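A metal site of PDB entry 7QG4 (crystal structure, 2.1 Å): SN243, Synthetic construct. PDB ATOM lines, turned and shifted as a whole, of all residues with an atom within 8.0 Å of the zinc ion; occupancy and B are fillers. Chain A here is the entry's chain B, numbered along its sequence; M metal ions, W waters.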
ATOM      1  N   SER A 235      11.216 -28.029   8.122  1.00  0.00           N
ATOM      2  CA  SER A 235      12.082 -27.988   6.949  1.00  0.00           C
ATOM      3  C   SER A 235      13.522 -27.691   7.312  1.00  0.00           C
ATOM      4  O   SER A 235      14.215 -26.954   6.619  1.00  0.00           O
ATOM      5  CB  SER A 235      11.569 -26.918   5.992  1.00  0.00           C
ATOM      6  OG  SER A 235      10.169 -26.843   5.990  1.00  0.00           O
ATOM      7  N   THR A 236      13.990 -28.252   8.419  1.00  0.00           N
ATOM      8  CA  THR A 236      15.333 -27.952   8.857  1.00  0.00           C
ATOM      9  C   THR A 236      16.366 -28.591   7.959  1.00  0.00           C
ATOM     10  O   THR A 236      17.434 -28.028   7.773  1.00  0.00           O
ATOM     11  CB  THR A 236      15.500 -28.389  10.308  1.00  0.00           C
ATOM     12  OG1 THR A 236      15.092 -29.751  10.451  1.00  0.00           O
ATOM     13  CG2 THR A 236      14.648 -27.514  11.236  1.00  0.00           C
ATOM     14  N   GLU A 237      16.044 -29.738   7.351  1.00  0.00           N
ATOM     15  CA  GLU A 237      16.976 -30.445   6.491  1.00  0.00           C
ATOM     16  C   GLU A 237      16.521 -30.416   5.043  1.00  0.00           C
ATOM     17  O   GLU A 237      15.647 -31.200   4.662  1.00  0.00           O
ATOM     18  CB  GLU A 237      17.153 -31.883   6.964  1.00  0.00           C
ATOM     19  CG  GLU A 237      17.886 -32.778   5.978  1.00  0.00           C
ATOM     20  CD  GLU A 237      19.262 -32.268   5.629  1.00  0.00           C
ATOM     21  OE1 GLU A 237      20.221 -32.597   6.370  1.00  0.00           O
ATOM     22  OE2 GLU A 237      19.404 -31.514   4.638  1.00  0.00           O
ATOM     23  N   PRO A 238      17.095 -29.573   4.197  1.00  0.00           N
ATOM     24  CA  PRO A 238      16.543 -29.409   2.840  1.00  0.00           C
ATOM     25  C   PRO A 238      16.613 -30.648   1.976  1.00  0.00           C
ATOM     26  O   PRO A 238      15.977 -30.678   0.921  1.00  0.00           O
ATOM     27  CB  PRO A 238      17.377 -28.261   2.264  1.00  0.00           C
ATOM     28  CG  PRO A 238      18.618 -28.229   3.093  1.00  0.00           C
ATOM     29  CD  PRO A 238      18.190 -28.635   4.468  1.00  0.00           C
ATOM     30  N   GLU A 249      10.421 -24.374   8.135  1.00  0.00           N
ATOM     31  CA  GLU A 249      11.568 -24.796   8.921  1.00  0.00           C
ATOM     32  C   GLU A 249      11.530 -24.246  10.339  1.00  0.00           C
ATOM     33  O   GLU A 249      12.124 -24.843  11.236  1.00  0.00           O
ATOM     34  CB  GLU A 249      12.853 -24.349   8.243  1.00  0.00           C
ATOM     35  CG  GLU A 249      13.012 -22.843   8.136  1.00  0.00           C
ATOM     36  CD  GLU A 249      14.379 -22.408   7.616  1.00  0.00           C
ATOM     37  OE1 GLU A 249      15.146 -23.278   7.149  1.00  0.00           O
ATOM     38  OE2 GLU A 249      14.687 -21.202   7.687  1.00  0.00           O
ATOM     39  N   GLY A 294      11.812 -33.872  10.804  1.00  0.00           N
ATOM     40  CA  GLY A 294      12.550 -32.991   9.935  1.00  0.00           C
ATOM     41  C   GLY A 294      14.037 -33.155   9.914  1.00  0.00           C
ATOM     42  O   GLY A 294      14.659 -33.030   8.855  1.00  0.00           O
ATOM     43  N   PRO A 295      14.709 -33.385  11.080  1.00  0.00           N
ATOM     44  CA  PRO A 295      16.179 -33.439  11.084  1.00  0.00           C
ATOM     45  C   PRO A 295      16.727 -34.820  10.751  1.00  0.00           C
ATOM     46  O   PRO A 295      17.203 -35.579  11.615  1.00  0.00           O
ATOM     47  CB  PRO A 295      16.514 -33.008  12.506  1.00  0.00           C
ATOM     48  CG  PRO A 295      15.407 -33.590  13.296  1.00  0.00           C
ATOM     49  CD  PRO A 295      14.181 -33.497  12.450  1.00  0.00           C
ATOM     50  N   PRO A 313      22.615 -31.906  15.377  1.00  0.00           N
ATOM     51  CA  PRO A 313      23.839 -31.124  15.611  1.00  0.00           C
ATOM     52  C   PRO A 313      23.658 -29.878  16.462  1.00  0.00           C
ATOM     53  O   PRO A 313      24.596 -29.481  17.155  1.00  0.00           O
ATOM     54  CB  PRO A 313      24.308 -30.758  14.199  1.00  0.00           C
ATOM     55  CG  PRO A 313      23.727 -31.806  13.336  1.00  0.00           C
ATOM     56  CD  PRO A 313      22.395 -32.157  13.949  1.00  0.00           C
ATOM     57  N   ALA A 314      22.516 -29.223  16.393  1.00  0.00           N
ATOM     58  CA  ALA A 314      22.255 -28.059  17.239  1.00  0.00           C
ATOM     59  C   ALA A 314      21.423 -28.393  18.467  1.00  0.00           C
ATOM     60  O   ALA A 314      20.902 -27.469  19.100  1.00  0.00           O
ATOM     61  CB  ALA A 314      21.579 -26.963  16.416  1.00  0.00           C
ATOM     62  N   ARG A 316      18.431 -29.507  18.901  1.00  0.00           N
ATOM     63  CA  ARG A 316      17.080 -28.891  18.823  1.00  0.00           C
ATOM     64  C   ARG A 316      15.996 -29.959  18.867  1.00  0.00           C
ATOM     65  O   ARG A 316      14.914 -29.700  18.408  1.00  0.00           O
ATOM     66  CB  ARG A 316      17.037 -28.026  17.577  1.00  0.00           C
ATOM     67  CG  ARG A 316      17.939 -26.810  17.684  1.00  0.00           C
ATOM     68  CD  ARG A 316      18.220 -26.179  16.355  1.00  0.00           C
ATOM     69  NE  ARG A 316      17.991 -24.752  16.334  1.00  0.00           N
ATOM     70  CZ  ARG A 316      18.887 -23.849  16.686  1.00  0.00           C
ATOM     71  NH1 ARG A 316      20.074 -24.216  17.098  1.00  0.00           N
ATOM     72  NH2 ARG A 316      18.586 -22.566  16.607  1.00  0.00           N
ATOM     73  N   HIS A 320      12.039 -29.237  17.956  1.00  0.00           N
ATOM     74  CA  HIS A 320      11.291 -29.928  16.931  1.00  0.00           C
ATOM     75  C   HIS A 320       9.961 -30.463  17.424  1.00  0.00           C
ATOM     76  O   HIS A 320       9.005 -30.534  16.659  1.00  0.00           O
ATOM     77  CB  HIS A 320      12.117 -31.068  16.337  1.00  0.00           C
ATOM     78  CG  HIS A 320      13.031 -30.619  15.257  1.00  0.00           C
ATOM     79  ND1 HIS A 320      12.761 -30.825  13.921  1.00  0.00           N
ATOM     80  CD2 HIS A 320      14.202 -29.950  15.297  1.00  0.00           C
ATOM     81  CE1 HIS A 320      13.729 -30.302  13.196  1.00  0.00           C
ATOM     82  NE2 HIS A 320      14.618 -29.776  14.010  1.00  0.00           N
ATOM     83  N   ALA A 725      26.681 -25.283   1.094  1.00  0.00           N
ATOM     84  CA  ALA A 725      25.867 -24.874   2.245  1.00  0.00           C
ATOM     85  C   ALA A 725      24.878 -25.983   2.592  1.00  0.00           C
ATOM     86  O   ALA A 725      24.565 -26.138   3.768  1.00  0.00           O
ATOM     87  CB  ALA A 725      25.166 -23.587   1.931  1.00  0.00           C
ATOM     88  N   ILE A 726      24.416 -26.724   1.584  1.00  0.00           N
ATOM     89  CA  ILE A 726      23.424 -27.812   1.796  1.00  0.00           C
ATOM     90  C   ILE A 726      24.079 -28.950   2.566  1.00  0.00           C
ATOM     91  O   ILE A 726      23.404 -29.583   3.376  1.00  0.00           O
ATOM     92  CB  ILE A 726      22.825 -28.287   0.459  1.00  0.00           C
ATOM     93  CG1 ILE A 726      22.030 -27.190  -0.229  1.00  0.00           C
ATOM     94  CG2 ILE A 726      22.006 -29.551   0.659  1.00  0.00           C
ATOM     95  CD1 ILE A 726      20.820 -26.742   0.548  1.00  0.00           C
ATOM     96  N   GLU A 728      26.890 -28.643   4.554  1.00  0.00           N
ATOM     97  CA  GLU A 728      27.439 -28.185   5.862  1.00  0.00           C
ATOM     98  C   GLU A 728      26.333 -27.814   6.832  1.00  0.00           C
ATOM     99  O   GLU A 728      26.546 -27.954   8.041  1.00  0.00           O
ATOM    100  CB  GLU A 728      28.354 -26.986   5.650  1.00  0.00           C
ATOM    101  CG  GLU A 728      29.100 -26.565   6.893  1.00  0.00           C
ATOM    102  CD  GLU A 728      30.212 -27.513   7.308  1.00  0.00           C
ATOM    103  OE1 GLU A 728      30.711 -28.243   6.446  1.00  0.00           O
ATOM    104  OE2 GLU A 728      30.565 -27.505   8.505  1.00  0.00           O
ATOM    105  N   GLN A 729      25.191 -27.358   6.332  1.00  0.00           N
ATOM    106  CA  GLN A 729      24.093 -26.894   7.217  1.00  0.00           C
ATOM    107  C   GLN A 729      23.753 -27.986   8.235  1.00  0.00           C
ATOM    108  O   GLN A 729      24.033 -29.154   7.948  1.00  0.00           O
ATOM    109  CB  GLN A 729      22.880 -26.472   6.394  1.00  0.00           C
ATOM    110  CG  GLN A 729      22.354 -27.562   5.485  1.00  0.00           C
ATOM    111  CD  GLN A 729      21.497 -28.554   6.210  1.00  0.00           C
ATOM    112  OE1 GLN A 729      20.816 -28.218   7.170  1.00  0.00           O
ATOM    113  NE2 GLN A 729      21.524 -29.791   5.761  1.00  0.00           N
ATOM    114  N   ASP A 730      23.179 -27.597   9.371  1.00  0.00           N
ATOM    115  CA  ASP A 730      22.844 -28.575  10.443  1.00  0.00           C
ATOM    116  C   ASP A 730      21.417 -29.104  10.218  1.00  0.00           C
ATOM    117  O   ASP A 730      20.513 -28.283   9.982  1.00  0.00           O
ATOM    118  CB  ASP A 730      23.095 -27.953  11.804  1.00  0.00           C
ATOM    119  CG  ASP A 730      24.512 -27.445  11.953  1.00  0.00           C
ATOM    120  OD1 ASP A 730      25.422 -28.152  11.513  1.00  0.00           O
ATOM    121  OD2 ASP A 730      24.684 -26.339  12.489  1.00  0.00           O
ATOM    122  N   SER A 731      21.226 -30.413  10.334  1.00  0.00           N
ATOM    123  CA  SER A 731      19.917 -31.031  10.007  1.00  0.00           C
ATOM    124  C   SER A 731      18.772 -30.502  10.861  1.00  0.00           C
ATOM    125  O   SER A 731      17.632 -30.585  10.386  1.00  0.00           O
ATOM    126  CB  SER A 731      20.014 -32.538  10.099  1.00  0.00           C
ATOM    127  OG  SER A 731      20.789 -33.055   9.041  1.00  0.00           O
ATOM    128  N   ASP A 732      19.024 -29.986  12.054  1.00  0.00           N
ATOM    129  CA  ASP A 732      17.934 -29.582  12.920  1.00  0.00           C
ATOM    130  C   ASP A 732      17.812 -28.081  13.081  1.00  0.00           C
ATOM    131  O   ASP A 732      17.050 -27.616  13.916  1.00  0.00           O
ATOM    132  CB  ASP A 732      18.061 -30.264  14.273  1.00  0.00           C
ATOM    133  CG  ASP A 732      19.416 -30.060  14.897  1.00  0.00           C
ATOM    134  OD1 ASP A 732      20.298 -29.469  14.241  1.00  0.00           O
ATOM    135  OD2 ASP A 732      19.592 -30.500  16.055  1.00  0.00           O
ATOM    136  N   ARG A 733      18.560 -27.322  12.312  1.00  0.00           N
ATOM    137  CA  ARG A 733      18.629 -25.885  12.453  1.00  0.00           C
ATOM    138  C   ARG A 733      18.043 -25.206  11.240  1.00  0.00           C
ATOM    139  O   ARG A 733      18.167 -25.725  10.135  1.00  0.00           O
ATOM    140  CB  ARG A 733      20.084 -25.460  12.647  1.00  0.00           C
ATOM    141  CG  ARG A 733      20.313 -23.980  12.830  1.00  0.00           C
ATOM    142  CD  ARG A 733      21.747 -23.670  12.531  1.00  0.00           C
ATOM    143  NE  ARG A 733      22.608 -24.687  13.112  1.00  0.00           N
ATOM    144  CZ  ARG A 733      23.170 -24.603  14.310  1.00  0.00           C
ATOM    145  NH1 ARG A 733      22.981 -23.527  15.054  1.00  0.00           N
ATOM    146  NH2 ARG A 733      23.937 -25.597  14.756  1.00  0.00           N
ATOM    147  N   PRO A 734      17.359 -24.087  11.413  1.00  0.00           N
ATOM    148  CA  PRO A 734      16.844 -23.355  10.258  1.00  0.00           C
ATOM    149  C   PRO A 734      17.930 -22.611   9.510  1.00  0.00           C
ATOM    150  O   PRO A 734      19.036 -22.404  10.010  1.00  0.00           O
ATOM    151  CB  PRO A 734      15.853 -22.365  10.868  1.00  0.00           C
ATOM    152  CG  PRO A 734      15.490 -22.974  12.185  1.00  0.00           C
ATOM    153  CD  PRO A 734      16.699 -23.698  12.659  1.00  0.00           C
ATOM    154  N   GLY A 735      17.613 -22.230   8.275  1.00  0.00           N
ATOM    155  CA  GLY A 735      18.489 -21.361   7.533  1.00  0.00           C
ATOM    156  C   GLY A 735      19.873 -21.938   7.241  1.00  0.00           C
ATOM    157  O   GLY A 735      20.185 -23.094   7.521  1.00  0.00           O
ATOM    158  N   TYR A 736      20.732 -21.043   6.733  1.00  0.00           N
ATOM    159  CA  TYR A 736      22.068 -21.409   6.321  1.00  0.00           C
ATOM    160  C   TYR A 736      23.115 -20.466   6.897  1.00  0.00           C
ATOM    161  O   TYR A 736      24.256 -20.432   6.419  1.00  0.00           O
ATOM    162  CB  TYR A 736      22.168 -21.450   4.794  1.00  0.00           C
ATOM    163  CG  TYR A 736      21.176 -22.406   4.149  1.00  0.00           C
ATOM    164  CD1 TYR A 736      21.447 -23.769   4.084  1.00  0.00           C
ATOM    165  CD2 TYR A 736      19.983 -21.947   3.628  1.00  0.00           C
ATOM    166  CE1 TYR A 736      20.544 -24.645   3.511  1.00  0.00           C
ATOM    167  CE2 TYR A 736      19.086 -22.827   3.043  1.00  0.00           C
ATOM    168  CZ  TYR A 736      19.367 -24.166   2.989  1.00  0.00           C
ATOM    169  OH  TYR A 736      18.477 -25.047   2.417  1.00  0.00           O
ATOM    170  N   ASP A 737      22.770 -19.733   7.950  1.00  0.00           N
ATOM    171  CA  ASP A 737      23.637 -18.695   8.485  1.00  0.00           C
ATOM    172  C   ASP A 737      24.879 -19.267   9.141  1.00  0.00           C
ATOM    173  O   ASP A 737      25.940 -18.659   9.079  1.00  0.00           O
ATOM    174  CB  ASP A 737      22.845 -17.836   9.454  1.00  0.00           C
ATOM    175  CG  ASP A 737      21.636 -17.169   8.796  1.00  0.00           C
ATOM    176  OD1 ASP A 737      21.501 -17.253   7.547  1.00  0.00           O
ATOM    177  OD2 ASP A 737      20.827 -16.577   9.535  1.00  0.00           O
ATOM    178  N   GLU A 738      24.752 -20.456   9.719  1.00  0.00           N
ATOM    179  CA  GLU A 738      25.909 -21.101  10.372  1.00  0.00           C
ATOM    180  C   GLU A 738      26.810 -21.739   9.312  1.00  0.00           C
ATOM    181  O   GLU A 738      27.685 -22.528   9.684  1.00  0.00           O
ATOM    182  CB  GLU A 738      25.445 -22.165  11.360  1.00  0.00           C
ATOM    183  CG  GLU A 738      25.056 -23.480  10.708  1.00  0.00           C
ATOM    184  CD  GLU A 738      23.776 -23.490   9.899  1.00  0.00           C
ATOM    185  OE1 GLU A 738      23.211 -22.409   9.674  1.00  0.00           O
ATOM    186  OE2 GLU A 738      23.341 -24.586   9.511  1.00  0.00           O
ATOM    187  N   THR A 739      26.597 -21.392   8.047  1.00  0.00           N
ATOM    188  CA  THR A 739      27.387 -22.008   6.957  1.00  0.00           C
ATOM    189  C   THR A 739      28.307 -20.949   6.359  1.00  0.00           C
ATOM    190  O   THR A 739      27.898 -19.777   6.291  1.00  0.00           O
ATOM    191  CB  THR A 739      26.492 -22.620   5.882  1.00  0.00           C
ATOM    192  OG1 THR A 739      25.910 -21.563   5.121  1.00  0.00           O
ATOM    193  CG2 THR A 739      25.415 -23.507   6.450  1.00  0.00           C
HETATM  194 ZN    ZN M   1      19.458 -26.853   8.774  1.00  0.00          ZN
HETATM  195  O   HOH W   1      19.359 -25.125   6.497  1.00  0.00           O
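The zinc ion is bound by the backbone carbonyl oxygen of Asp 730 (2.1 Å), the backbone carbonyl oxygen of Arg 733 (2.2 Å), the side-chain amide oxygen of Gln 729 (2.5 Å) and the backbone carbonyl oxygen of Thr 236 (2.5 Å).
The side-chain amide nitrogen of Gln 729 sits at hydrogen-bond distance from the backbone carbonyl oxygen of Ile 726 (3.0 Å).
The side-chain amide nitrogen of Gln 729 lies within hydrogen-bond range of the side-chain carboxylate of Glu 237 (3.0 Å).
O of Ser 731 is in hydrogen-bond range of OG1 of Thr 236 (2.7 Å).
The side-chain carboxylate (OD2) of Asp 730 lies within salt-bridge range of the guanidinium group (NH2) of Arg 733, at 2.5 Å.
The guanidinium group (NE) of Arg 733 is in salt-bridge range of the side-chain carboxylate (OE2) of Glu 738.
The backbone NH of Asp 730 sits at hydrogen-bond distance from the side-chain carboxylate of Glu 738, at 3.0 Å.
Within 4 Å of the zinc ion: Thr 236, Gln 729, Asp 730 and Arg 733.
The nearest printed residue that does not touch the zinc ion is Gly 735 (4.03 Å).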
